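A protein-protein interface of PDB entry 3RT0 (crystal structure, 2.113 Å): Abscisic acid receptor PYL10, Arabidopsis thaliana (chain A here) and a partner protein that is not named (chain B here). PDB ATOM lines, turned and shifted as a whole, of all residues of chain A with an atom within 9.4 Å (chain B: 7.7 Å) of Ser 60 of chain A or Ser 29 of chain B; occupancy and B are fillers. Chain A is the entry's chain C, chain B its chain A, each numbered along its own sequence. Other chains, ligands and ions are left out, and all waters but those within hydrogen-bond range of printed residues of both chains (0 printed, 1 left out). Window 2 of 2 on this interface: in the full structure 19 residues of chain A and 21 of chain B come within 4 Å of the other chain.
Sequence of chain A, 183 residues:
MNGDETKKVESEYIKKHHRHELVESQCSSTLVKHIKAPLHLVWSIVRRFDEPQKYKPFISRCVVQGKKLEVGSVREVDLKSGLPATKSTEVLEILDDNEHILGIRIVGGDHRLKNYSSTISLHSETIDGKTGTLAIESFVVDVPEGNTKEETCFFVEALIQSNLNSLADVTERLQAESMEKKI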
ATOM      1  N   PRO A  52       3.488  -5.570  31.208  1.00  0.00           N
ATOM      2  CA  PRO A  52       2.670  -6.396  32.099  1.00  0.00           C
ATOM      3  C   PRO A  52       2.121  -7.639  31.384  1.00  0.00           C
ATOM      4  O   PRO A  52       1.752  -8.589  32.072  1.00  0.00           O
ATOM      5  CB  PRO A  52       1.539  -5.450  32.522  1.00  0.00           C
ATOM      6  CG  PRO A  52       1.416  -4.497  31.376  1.00  0.00           C
ATOM      7  CD  PRO A  52       2.858  -4.265  30.942  1.00  0.00           C
ATOM      8  N   GLN A  53       2.077  -7.638  30.059  1.00  0.00           N
ATOM      9  CA  GLN A  53       1.562  -8.791  29.330  1.00  0.00           C
ATOM     10  C   GLN A  53       2.448 -10.021  29.514  1.00  0.00           C
ATOM     11  O   GLN A  53       2.094 -11.116  29.088  1.00  0.00           O
ATOM     12  CB  GLN A  53       1.387  -8.468  27.845  1.00  0.00           C
ATOM     13  CG  GLN A  53       2.681  -8.201  27.110  1.00  0.00           C
ATOM     14  CD  GLN A  53       3.053  -6.732  27.098  1.00  0.00           C
ATOM     15  OE1 GLN A  53       3.675  -6.250  26.158  1.00  0.00           O
ATOM     16  NE2 GLN A  53       2.672  -6.016  28.144  1.00  0.00           N
ATOM     17  N   LYS A  54       3.599  -9.839  30.155  1.00  0.00           N
ATOM     18  CA  LYS A  54       4.484 -10.965  30.437  1.00  0.00           C
ATOM     19  C   LYS A  54       3.781 -11.973  31.343  1.00  0.00           C
ATOM     20  O   LYS A  54       4.126 -13.151  31.362  1.00  0.00           O
ATOM     21  CB  LYS A  54       5.771 -10.488  31.104  1.00  0.00           C
ATOM     22  CG  LYS A  54       6.835  -9.974  30.156  1.00  0.00           C
ATOM     23  CD  LYS A  54       7.908  -9.209  30.927  1.00  0.00           C
ATOM     24  CE  LYS A  54       9.308  -9.591  30.466  1.00  0.00           C
ATOM     25  NZ  LYS A  54       9.499  -9.438  28.997  1.00  0.00           N
ATOM     26  N   LYS A  56       0.262 -10.782  33.066  1.00  0.00           N
ATOM     27  CA  LYS A  56      -1.139 -10.412  33.264  1.00  0.00           C
ATOM     28  C   LYS A  56      -1.953 -10.930  32.083  1.00  0.00           C
ATOM     29  O   LYS A  56      -1.798 -10.455  30.945  1.00  0.00           O
ATOM     30  CB  LYS A  56      -1.291  -8.902  33.442  1.00  0.00           C
ATOM     31  CG  LYS A  56      -0.563  -8.362  34.670  1.00  0.00           C
ATOM     32  CD  LYS A  56      -1.154  -7.037  35.130  1.00  0.00           C
ATOM     33  CE  LYS A  56      -0.477  -6.541  36.391  1.00  0.00           C
ATOM     34  NZ  LYS A  56      -1.136  -5.293  36.879  1.00  0.00           N
ATOM     35  N   PRO A  57      -2.828 -11.918  32.347  1.00  0.00           N
ATOM     36  CA  PRO A  57      -3.477 -12.686  31.264  1.00  0.00           C
ATOM     37  C   PRO A  57      -4.565 -11.930  30.490  1.00  0.00           C
ATOM     38  O   PRO A  57      -4.926 -12.349  29.387  1.00  0.00           O
ATOM     39  CB  PRO A  57      -4.076 -13.901  31.995  1.00  0.00           C
ATOM     40  CG  PRO A  57      -4.331 -13.386  33.399  1.00  0.00           C
ATOM     41  CD  PRO A  57      -3.184 -12.424  33.683  1.00  0.00           C
ATOM     42  N   PHE A  58      -5.071 -10.827  31.029  1.00  0.00           N
ATOM     43  CA  PHE A  58      -6.115 -10.099  30.318  1.00  0.00           C
ATOM     44  C   PHE A  58      -5.613  -8.961  29.413  1.00  0.00           C
ATOM     45  O   PHE A  58      -6.415  -8.287  28.773  1.00  0.00           O
ATOM     46  CB  PHE A  58      -7.172  -9.582  31.297  1.00  0.00           C
ATOM     47  CG  PHE A  58      -8.065 -10.664  31.836  1.00  0.00           C
ATOM     48  CD1 PHE A  58      -8.931 -11.341  30.993  1.00  0.00           C
ATOM     49  CD2 PHE A  58      -8.031 -11.008  33.174  1.00  0.00           C
ATOM     50  CE1 PHE A  58      -9.761 -12.345  31.483  1.00  0.00           C
ATOM     51  CE2 PHE A  58      -8.850 -12.005  33.668  1.00  0.00           C
ATOM     52  CZ  PHE A  58      -9.715 -12.674  32.819  1.00  0.00           C
ATOM     53  N   ILE A  59      -4.300  -8.747  29.360  1.00  0.00           N
ATOM     54  CA  ILE A  59      -3.758  -7.636  28.573  1.00  0.00           C
ATOM     55  C   ILE A  59      -3.446  -8.033  27.137  1.00  0.00           C
ATOM     56  O   ILE A  59      -2.610  -8.892  26.894  1.00  0.00           O
ATOM     57  CB  ILE A  59      -2.510  -7.036  29.230  1.00  0.00           C
ATOM     58  CG1 ILE A  59      -2.872  -6.501  30.619  1.00  0.00           C
ATOM     59  CG2 ILE A  59      -1.914  -5.940  28.321  1.00  0.00           C
ATOM     60  CD1 ILE A  59      -1.801  -5.697  31.273  1.00  0.00           C
ATOM     61  N   SER A  60      -4.135  -7.412  26.185  1.00  0.00           N
ATOM     62  CA  SER A  60      -3.894  -7.721  24.784  1.00  0.00           C
ATOM     63  C   SER A  60      -2.795  -6.834  24.240  1.00  0.00           C
ATOM     64  O   SER A  60      -2.074  -7.227  23.331  1.00  0.00           O
ATOM     65  CB  SER A  60      -5.153  -7.548  23.951  1.00  0.00           C
ATOM     66  OG  SER A  60      -5.548  -6.201  23.933  1.00  0.00           O
ATOM     67  N   ARG A  61      -2.664  -5.631  24.783  1.00  0.00           N
ATOM     68  CA  ARG A  61      -1.658  -4.700  24.291  1.00  0.00           C
ATOM     69  C   ARG A  61      -1.266  -3.678  25.345  1.00  0.00           C
ATOM     70  O   ARG A  61      -2.097  -3.241  26.138  1.00  0.00           O
ATOM     71  CB  ARG A  61      -2.163  -3.990  23.033  1.00  0.00           C
ATOM     72  CG  ARG A  61      -1.188  -2.982  22.457  1.00  0.00           C
ATOM     73  CD  ARG A  61      -1.913  -1.833  21.776  1.00  0.00           C
ATOM     74  NE  ARG A  61      -2.424  -2.213  20.465  1.00  0.00           N
ATOM     75  CZ  ARG A  61      -1.967  -1.728  19.315  1.00  0.00           C
ATOM     76  NH1 ARG A  61      -0.983  -0.839  19.313  1.00  0.00           N
ATOM     77  NH2 ARG A  61      -2.495  -2.131  18.167  1.00  0.00           N
ATOM     78  N   CYS A  62       0.004  -3.293  25.351  1.00  0.00           N
ATOM     79  CA  CYS A  62       0.464  -2.272  26.288  1.00  0.00           C
ATOM     80  C   CYS A  62       1.476  -1.324  25.641  1.00  0.00           C
ATOM     81  O   CYS A  62       2.491  -1.751  25.100  1.00  0.00           O
ATOM     82  CB  CYS A  62       1.072  -2.919  27.530  1.00  0.00           C
ATOM     83  SG  CYS A  62       1.638  -1.734  28.761  1.00  0.00           S
ATOM     84  N   VAL A  63       1.194  -0.029  25.712  1.00  0.00           N
ATOM     85  CA  VAL A  63       2.042   0.981  25.088  1.00  0.00           C
ATOM     86  C   VAL A  63       2.492   1.992  26.137  1.00  0.00           C
ATOM     87  O   VAL A  63       1.667   2.557  26.864  1.00  0.00           O
ATOM     88  CB  VAL A  63       1.276   1.723  23.984  1.00  0.00           C
ATOM     89  CG1 VAL A  63       2.049   2.952  23.540  1.00  0.00           C
ATOM     90  CG2 VAL A  63       0.993   0.794  22.813  1.00  0.00           C
ATOM     91  N   GLU A  76      -0.460   2.618  28.671  1.00  0.00           N
ATOM     92  CA  GLU A  76      -1.802   2.505  28.126  1.00  0.00           C
ATOM     93  C   GLU A  76      -2.086   1.047  27.779  1.00  0.00           C
ATOM     94  O   GLU A  76      -1.407   0.441  26.957  1.00  0.00           O
ATOM     95  CB  GLU A  76      -1.952   3.364  26.862  1.00  0.00           C
ATOM     96  CG  GLU A  76      -2.833   4.612  27.019  1.00  0.00           C
ATOM     97  CD  GLU A  76      -4.144   4.337  27.751  1.00  0.00           C
ATOM     98  OE1 GLU A  76      -5.120   3.847  27.126  1.00  0.00           O
ATOM     99  OE2 GLU A  76      -4.198   4.616  28.965  1.00  0.00           O
ATOM    100  N   VAL A  77      -3.109   0.492  28.403  1.00  0.00           N
ATOM    101  CA  VAL A  77      -3.382  -0.920  28.258  1.00  0.00           C
ATOM    102  C   VAL A  77      -4.701  -1.146  27.541  1.00  0.00           C
ATOM    103  O   VAL A  77      -5.695  -0.498  27.845  1.00  0.00           O
ATOM    104  CB  VAL A  77      -3.418  -1.599  29.632  1.00  0.00           C
ATOM    105  CG1 VAL A  77      -4.000  -2.990  29.518  1.00  0.00           C
ATOM    106  CG2 VAL A  77      -2.009  -1.628  30.251  1.00  0.00           C
ATOM    107  N   ASP A  78      -4.688  -2.046  26.566  1.00  0.00           N
ATOM    108  CA  ASP A  78      -5.910  -2.555  25.966  1.00  0.00           C
ATOM    109  C   ASP A  78      -6.160  -3.961  26.485  1.00  0.00           C
ATOM    110  O   ASP A  78      -5.230  -4.777  26.583  1.00  0.00           O
ATOM    111  CB  ASP A  78      -5.799  -2.580  24.447  1.00  0.00           C
ATOM    112  CG  ASP A  78      -5.928  -1.208  23.842  1.00  0.00           C
ATOM    113  OD1 ASP A  78      -4.884  -0.548  23.640  1.00  0.00           O
ATOM    114  OD2 ASP A  78      -7.078  -0.783  23.580  1.00  0.00           O
ATOM    115  N   LEU A  79      -7.415  -4.245  26.818  1.00  0.00           N
ATOM    116  CA  LEU A  79      -7.752  -5.503  27.452  1.00  0.00           C
ATOM    117  C   LEU A  79      -8.379  -6.463  26.452  1.00  0.00           C
ATOM    118  O   LEU A  79      -8.958  -6.045  25.452  1.00  0.00           O
ATOM    119  CB  LEU A  79      -8.708  -5.262  28.624  1.00  0.00           C
ATOM    120  CG  LEU A  79      -8.212  -4.325  29.732  1.00  0.00           C
ATOM    121  CD1 LEU A  79      -9.336  -3.941  30.664  1.00  0.00           C
ATOM    122  CD2 LEU A  79      -7.085  -4.986  30.514  1.00  0.00           C
ATOM    123  N   LYS A  80      -8.254  -7.754  26.727  1.00  0.00           N
ATOM    124  CA  LYS A  80      -8.939  -8.773  25.940  1.00  0.00           C
ATOM    125  C   LYS A  80     -10.444  -8.732  26.228  1.00  0.00           C
ATOM    126  O   LYS A  80     -10.874  -8.205  27.263  1.00  0.00           O
ATOM    127  CB  LYS A  80      -8.341 -10.151  26.247  1.00  0.00           C
ATOM    128  CG  LYS A  80      -6.889 -10.280  25.767  1.00  0.00           C
ATOM    129  CD  LYS A  80      -6.214 -11.563  26.227  1.00  0.00           C
ATOM    130  CE  LYS A  80      -4.754 -11.603  25.759  1.00  0.00           C
ATOM    131  NZ  LYS A  80      -3.971 -12.747  26.321  1.00  0.00           N
ATOM    132  N   SER A  81     -11.249  -9.279  25.322  1.00  0.00           N
ATOM    133  CA  SER A  81     -12.700  -9.194  25.476  1.00  0.00           C
ATOM    134  C   SER A  81     -13.217 -10.025  26.654  1.00  0.00           C
ATOM    135  O   SER A  81     -12.557 -10.965  27.106  1.00  0.00           O
ATOM    136  CB  SER A  81     -13.421  -9.580  24.184  1.00  0.00           C
ATOM    137  OG  SER A  81     -13.481 -10.982  24.047  1.00  0.00           O
ATOM    138  N   LEU A  83     -14.214  -8.644  29.745  1.00  0.00           N
ATOM    139  CA  LEU A  83     -14.205  -7.839  30.958  1.00  0.00           C
ATOM    140  C   LEU A  83     -15.190  -6.692  30.850  1.00  0.00           C
ATOM    141  O   LEU A  83     -15.570  -6.299  29.751  1.00  0.00           O
ATOM    142  CB  LEU A  83     -12.816  -7.254  31.170  1.00  0.00           C
ATOM    143  CG  LEU A  83     -11.921  -7.984  32.163  1.00  0.00           C
ATOM    144  CD1 LEU A  83     -12.381  -9.416  32.344  1.00  0.00           C
ATOM    145  CD2 LEU A  83     -10.485  -7.922  31.682  1.00  0.00           C
ATOM    146  N   ALA A  85     -14.585  -3.722  30.832  1.00  0.00           N
ATOM    147  CA  ALA A  85     -13.642  -2.640  30.574  1.00  0.00           C
ATOM    148  C   ALA A  85     -12.881  -3.016  29.313  1.00  0.00           C
ATOM    149  O   ALA A  85     -12.828  -4.182  28.962  1.00  0.00           O
ATOM    150  CB  ALA A  85     -12.686  -2.485  31.742  1.00  0.00           C
ATOM    151  N   THR A  86     -12.309  -2.047  28.613  1.00  0.00           N
ATOM    152  CA  THR A  86     -11.555  -2.372  27.407  1.00  0.00           C
ATOM    153  C   THR A  86     -10.176  -1.734  27.402  1.00  0.00           C
ATOM    154  O   THR A  86      -9.298  -2.149  26.646  1.00  0.00           O
ATOM    155  CB  THR A  86     -12.286  -1.935  26.142  1.00  0.00           C
ATOM    156  OG1 THR A  86     -12.349  -0.507  26.101  1.00  0.00           O
ATOM    157  CG2 THR A  86     -13.693  -2.495  26.121  1.00  0.00           C
ATOM    158  N   LYS A  87      -9.994  -0.715  28.233  1.00  0.00           N
ATOM    159  CA  LYS A  87      -8.706  -0.018  28.311  1.00  0.00           C
ATOM    160  C   LYS A  87      -8.481   0.620  29.671  1.00  0.00           C
ATOM    161  O   LYS A  87      -9.419   0.843  30.436  1.00  0.00           O
ATOM    162  CB  LYS A  87      -8.581   1.044  27.211  1.00  0.00           C
ATOM    163  CG  LYS A  87      -9.719   2.069  27.179  1.00  0.00           C
ATOM    164  CD  LYS A  87      -9.670   2.900  25.896  1.00  0.00           C
ATOM    165  CE  LYS A  87     -10.382   4.241  26.053  1.00  0.00           C
ATOM    166  NZ  LYS A  87     -11.782   4.117  26.539  1.00  0.00           N
ATOM    167  N   GLN B  25     -12.195  -9.027  12.630  1.00  0.00           N
ATOM    168  CA  GLN B  25     -11.715  -8.479  13.899  1.00  0.00           C
ATOM    169  C   GLN B  25     -12.483  -7.218  14.237  1.00  0.00           C
ATOM    170  O   GLN B  25     -12.716  -6.913  15.400  1.00  0.00           O
ATOM    171  CB  GLN B  25     -10.212  -8.179  13.794  1.00  0.00           C
ATOM    172  CG  GLN B  25      -9.577  -7.550  15.021  1.00  0.00           C
ATOM    173  CD  GLN B  25      -8.051  -7.572  14.938  1.00  0.00           C
ATOM    174  OE1 GLN B  25      -7.486  -8.141  14.008  1.00  0.00           O
ATOM    175  NE2 GLN B  25      -7.385  -6.960  15.912  1.00  0.00           N
ATOM    176  N   GLY B  26     -12.885  -6.487  13.206  1.00  0.00           N
ATOM    177  CA  GLY B  26     -13.599  -5.241  13.401  1.00  0.00           C
ATOM    178  C   GLY B  26     -12.792  -4.229  14.198  1.00  0.00           C
ATOM    179  O   GLY B  26     -11.560  -4.171  14.101  1.00  0.00           O
ATOM    180  N   ASN B  27     -13.490  -3.442  15.010  1.00  0.00           N
ATOM    181  CA  ASN B  27     -12.858  -2.354  15.750  1.00  0.00           C
ATOM    182  C   ASN B  27     -12.088  -2.798  17.000  1.00  0.00           C
ATOM    183  O   ASN B  27     -11.731  -1.971  17.838  1.00  0.00           O
ATOM    184  CB  ASN B  27     -13.893  -1.282  16.115  1.00  0.00           C
ATOM    185  CG  ASN B  27     -14.608  -0.714  14.891  1.00  0.00           C
ATOM    186  OD1 ASN B  27     -15.833  -0.571  14.888  1.00  0.00           O
ATOM    187  ND2 ASN B  27     -13.845  -0.395  13.846  1.00  0.00           N
ATOM    188  N   ARG B  28     -11.835  -4.096  17.114  1.00  0.00           N
ATOM    189  CA  ARG B  28     -11.154  -4.650  18.279  1.00  0.00           C
ATOM    190  C   ARG B  28      -9.637  -4.698  18.104  1.00  0.00           C
ATOM    191  O   ARG B  28      -9.131  -4.691  16.985  1.00  0.00           O
ATOM    192  CB  ARG B  28     -11.680  -6.049  18.587  1.00  0.00           C
ATOM    193  CG  ARG B  28     -12.856  -6.071  19.539  1.00  0.00           C
ATOM    194  CD  ARG B  28     -12.518  -6.819  20.815  1.00  0.00           C
ATOM    195  NE  ARG B  28     -12.800  -6.017  22.000  1.00  0.00           N
ATOM    196  CZ  ARG B  28     -12.071  -6.042  23.107  1.00  0.00           C
ATOM    197  NH1 ARG B  28     -12.400  -5.278  24.137  1.00  0.00           N
ATOM    198  NH2 ARG B  28     -11.012  -6.836  23.186  1.00  0.00           N
ATOM    199  N   SER B  29      -8.926  -4.761  19.225  1.00  0.00           N
ATOM    200  CA  SER B  29      -7.467  -4.795  19.222  1.00  0.00           C
ATOM    201  C   SER B  29      -6.902  -6.166  18.849  1.00  0.00           C
ATOM    202  O   SER B  29      -5.738  -6.279  18.470  1.00  0.00           O
ATOM    203  CB  SER B  29      -6.924  -4.357  20.584  1.00  0.00           C
ATOM    204  OG  SER B  29      -5.574  -4.751  20.750  1.00  0.00           O
ATOM    205  N   GLU B  30      -7.728  -7.202  18.960  1.00  0.00           N
ATOM    206  CA  GLU B  30      -7.319  -8.555  18.583  1.00  0.00           C
ATOM    207  C   GLU B  30      -8.517  -9.468  18.302  1.00  0.00           C
ATOM    208  O   GLU B  30      -9.616  -9.238  18.798  1.00  0.00           O
ATOM    209  CB  GLU B  30      -6.388  -9.166  19.636  1.00  0.00           C
ATOM    210  CG  GLU B  30      -7.059  -9.569  20.935  1.00  0.00           C
ATOM    211  CD  GLU B  30      -6.184 -10.488  21.777  1.00  0.00           C
ATOM    212  OE1 GLU B  30      -6.692 -11.525  22.255  1.00  0.00           O
ATOM    213  OE2 GLU B  30      -4.988 -10.175  21.959  1.00  0.00           O
ATOM    214  N   MET B  31      -8.298 -10.488  17.480  1.00  0.00           N
ATOM    215  CA  MET B  31      -9.365 -11.394  17.071  1.00  0.00           C
ATOM    216  C   MET B  31      -9.528 -12.550  18.049  1.00  0.00           C
ATOM    217  O   MET B  31      -8.603 -13.326  18.268  1.00  0.00           O
ATOM    218  CB  MET B  31      -9.100 -11.927  15.661  1.00  0.00           C
ATOM    219  CG  MET B  31     -10.201 -12.818  15.103  1.00  0.00           C
ATOM    220  SD  MET B  31     -11.834 -12.062  15.144  1.00  0.00           S
ATOM    221  CE  MET B  31     -12.622 -12.877  13.764  1.00  0.00           C
ATOM    222  N   GLU B  32     -10.713 -12.657  18.637  1.00  0.00           N
ATOM    223  CA  GLU B  32     -11.002 -13.720  19.589  1.00  0.00           C
ATOM    224  C   GLU B  32     -12.213 -14.546  19.152  1.00  0.00           C
ATOM    225  O   GLU B  32     -12.715 -15.369  19.907  1.00  0.00           O
ATOM    226  CB  GLU B  32     -11.225 -13.143  20.988  1.00  0.00           C
ATOM    227  CG  GLU B  32      -9.947 -12.759  21.716  1.00  0.00           C
ATOM    228  CD  GLU B  32     -10.205 -11.941  22.967  1.00  0.00           C
ATOM    229  OE1 GLU B  32     -10.777 -12.483  23.932  1.00  0.00           O
ATOM    230  OE2 GLU B  32      -9.836 -10.753  22.986  1.00  0.00           O
ATOM    231  N   LYS B 320     -18.132  -2.309  18.496  1.00  0.00           N
ATOM    232  CA  LYS B 320     -16.698  -2.261  18.756  1.00  0.00           C
ATOM    233  C   LYS B 320     -16.153  -3.641  19.159  1.00  0.00           C
ATOM    234  O   LYS B 320     -15.284  -3.755  20.026  1.00  0.00           O
ATOM    235  CB  LYS B 320     -16.391  -1.209  19.832  1.00  0.00           C
ATOM    236  CG  LYS B 320     -17.597  -0.841  20.702  1.00  0.00           C
ATOM    237  CD  LYS B 320     -17.487  -1.412  22.112  1.00  0.00           C
ATOM    238  CE  LYS B 320     -17.124  -0.336  23.134  1.00  0.00           C
ATOM    239  NZ  LYS B 320     -15.768   0.243  22.913  1.00  0.00           N
ATOM    240  N   ASP B 321     -16.662  -4.686  18.513  1.00  0.00           N
ATOM    241  CA  ASP B 321     -16.298  -6.056  18.869  1.00  0.00           C
ATOM    242  C   ASP B 321     -15.972  -6.904  17.638  1.00  0.00           C
ATOM    243  O   ASP B 321     -16.236  -6.490  16.509  1.00  0.00           O
ATOM    244  CB  ASP B 321     -17.453  -6.692  19.621  1.00  0.00           C
ATOM    245  CG  ASP B 321     -17.025  -7.886  20.429  1.00  0.00           C
ATOM    246  OD1 ASP B 321     -15.836  -8.291  20.331  1.00  0.00           O
ATOM    247  OD2 ASP B 321     -17.881  -8.411  21.170  1.00  0.00           O
ATOM    248  N   ASN B 322     -15.403  -8.089  17.847  1.00  0.00           N
ATOM    249  CA  ASN B 322     -15.303  -9.043  16.755  1.00  0.00           C
ATOM    250  C   ASN B 322     -16.705  -9.420  16.288  1.00  0.00           C
ATOM    251  O   ASN B 322     -17.623  -9.541  17.087  1.00  0.00           O
ATOM    252  CB  ASN B 322     -14.544 -10.304  17.163  1.00  0.00           C
ATOM    253  CG  ASN B 322     -13.201 -10.008  17.824  1.00  0.00           C
ATOM    254  OD1 ASN B 322     -12.809 -10.688  18.774  1.00  0.00           O
ATOM    255  ND2 ASN B 322     -12.491  -9.009  17.319  1.00  0.00           N
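Ser 60 of chain A touches Glu 30 of chain B. Lys 80 of chain A touches Arg 28 of chain B. Glu 30 of chain B touches Lys 80 of chain A (OE1 to CG, 3.7 Å). OE2 of Glu 32 of chain B touches CB of Lys 80 of chain A (3.6 Å). Thr 86 of chain A touches Arg 28 of chain B.
Of the 21 printed residues of chain A, 5 touch a printed residue of chain B. Among the printed residues, 9 pairs touch across the chains.
Lys 56 of chain A touches none of the printed residues of chain B. Of the printed residues of chain B, Lys 80 of chain A touches Arg 28 (3.6 Å), Glu 30 (3.7 Å) and Glu 32 (3.6 Å). Of the printed residues of chain B, Ser 81 of chain A touches Arg 28 and Glu 32. Printed residues of chain B within 4 Å of Thr 86 of chain A: Arg 28 (3.7 Å). Of the printed residues of chain A, Arg 28 of chain B touches Leu 79 (3.2 Å), Lys 80 (3.6 Å), Ser 81 (3.3 Å) and Thr 86 (3.7 Å). Of the printed residues of chain A, Ser 29 of chain B touches Ser 60. Glu 30 of chain B touches just these residues of chain A: Ser 60 (3.3 Å) and Lys 80 (3.7 Å). Printed residues of chain A within 4 Å of Glu 32 of chain B: Lys 80 and Ser 81. The nearest residue of chain B that does not touch Ser 60 of chain A is Arg 28 of chain B (5.6 Å). The nearest printed residue of chain B that does not touch Lys 80 of chain A is Ser 29 of chain B (7.1 Å).
N of Ser 81 of chain A sits close to NH2 of Arg 28 of chain B (3.3 Å). The side-chain hydroxyl (OG) of Ser 81 of chain A lies within hydrogen-bond range of the side-chain carboxylate (OE1) of Glu 32 of chain B. NH2 of Arg 28 of chain B sits at hydrogen-bond distance from O of Leu 79 of chain A (3.2 Å). The side-chain hydroxyl of Ser 60 of chain A is in hydrogen-bond range of the side-chain hydroxyl of Ser 29 of chain B (3.5 Å).
N of Glu 30 of chain B sits close to NE2 of Gln 25 of chain B (3.1 Å). The backbone carbonyl oxygen (O) of Glu 30 of chain B sits at hydrogen-bond distance from the side-chain amide nitrogen (ND2) of Asn 322 of chain B (3.2 Å). The backbone carbonyl oxygen of Phe 58 of chain A is in hydrogen-bond range of the backbone NH of Lys 80 of chain A (2.8 Å). The side-chain amide oxygen (OD1) of Asn 322 of chain B lies within hydrogen-bond range of the backbone NH (N) of Glu 32 of chain B. The backbone carbonyl oxygen (O) of Asp 78 of chain A lies within hydrogen-bond range of the backbone NH (N) of Ser 60 of chain A (2.9 Å). The backbone carbonyl oxygen (O) of Arg 28 of chain B lies within hydrogen-bond range of the side-chain amide nitrogen (NE2) of Gln 25 of chain B, 3.1 Å away.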
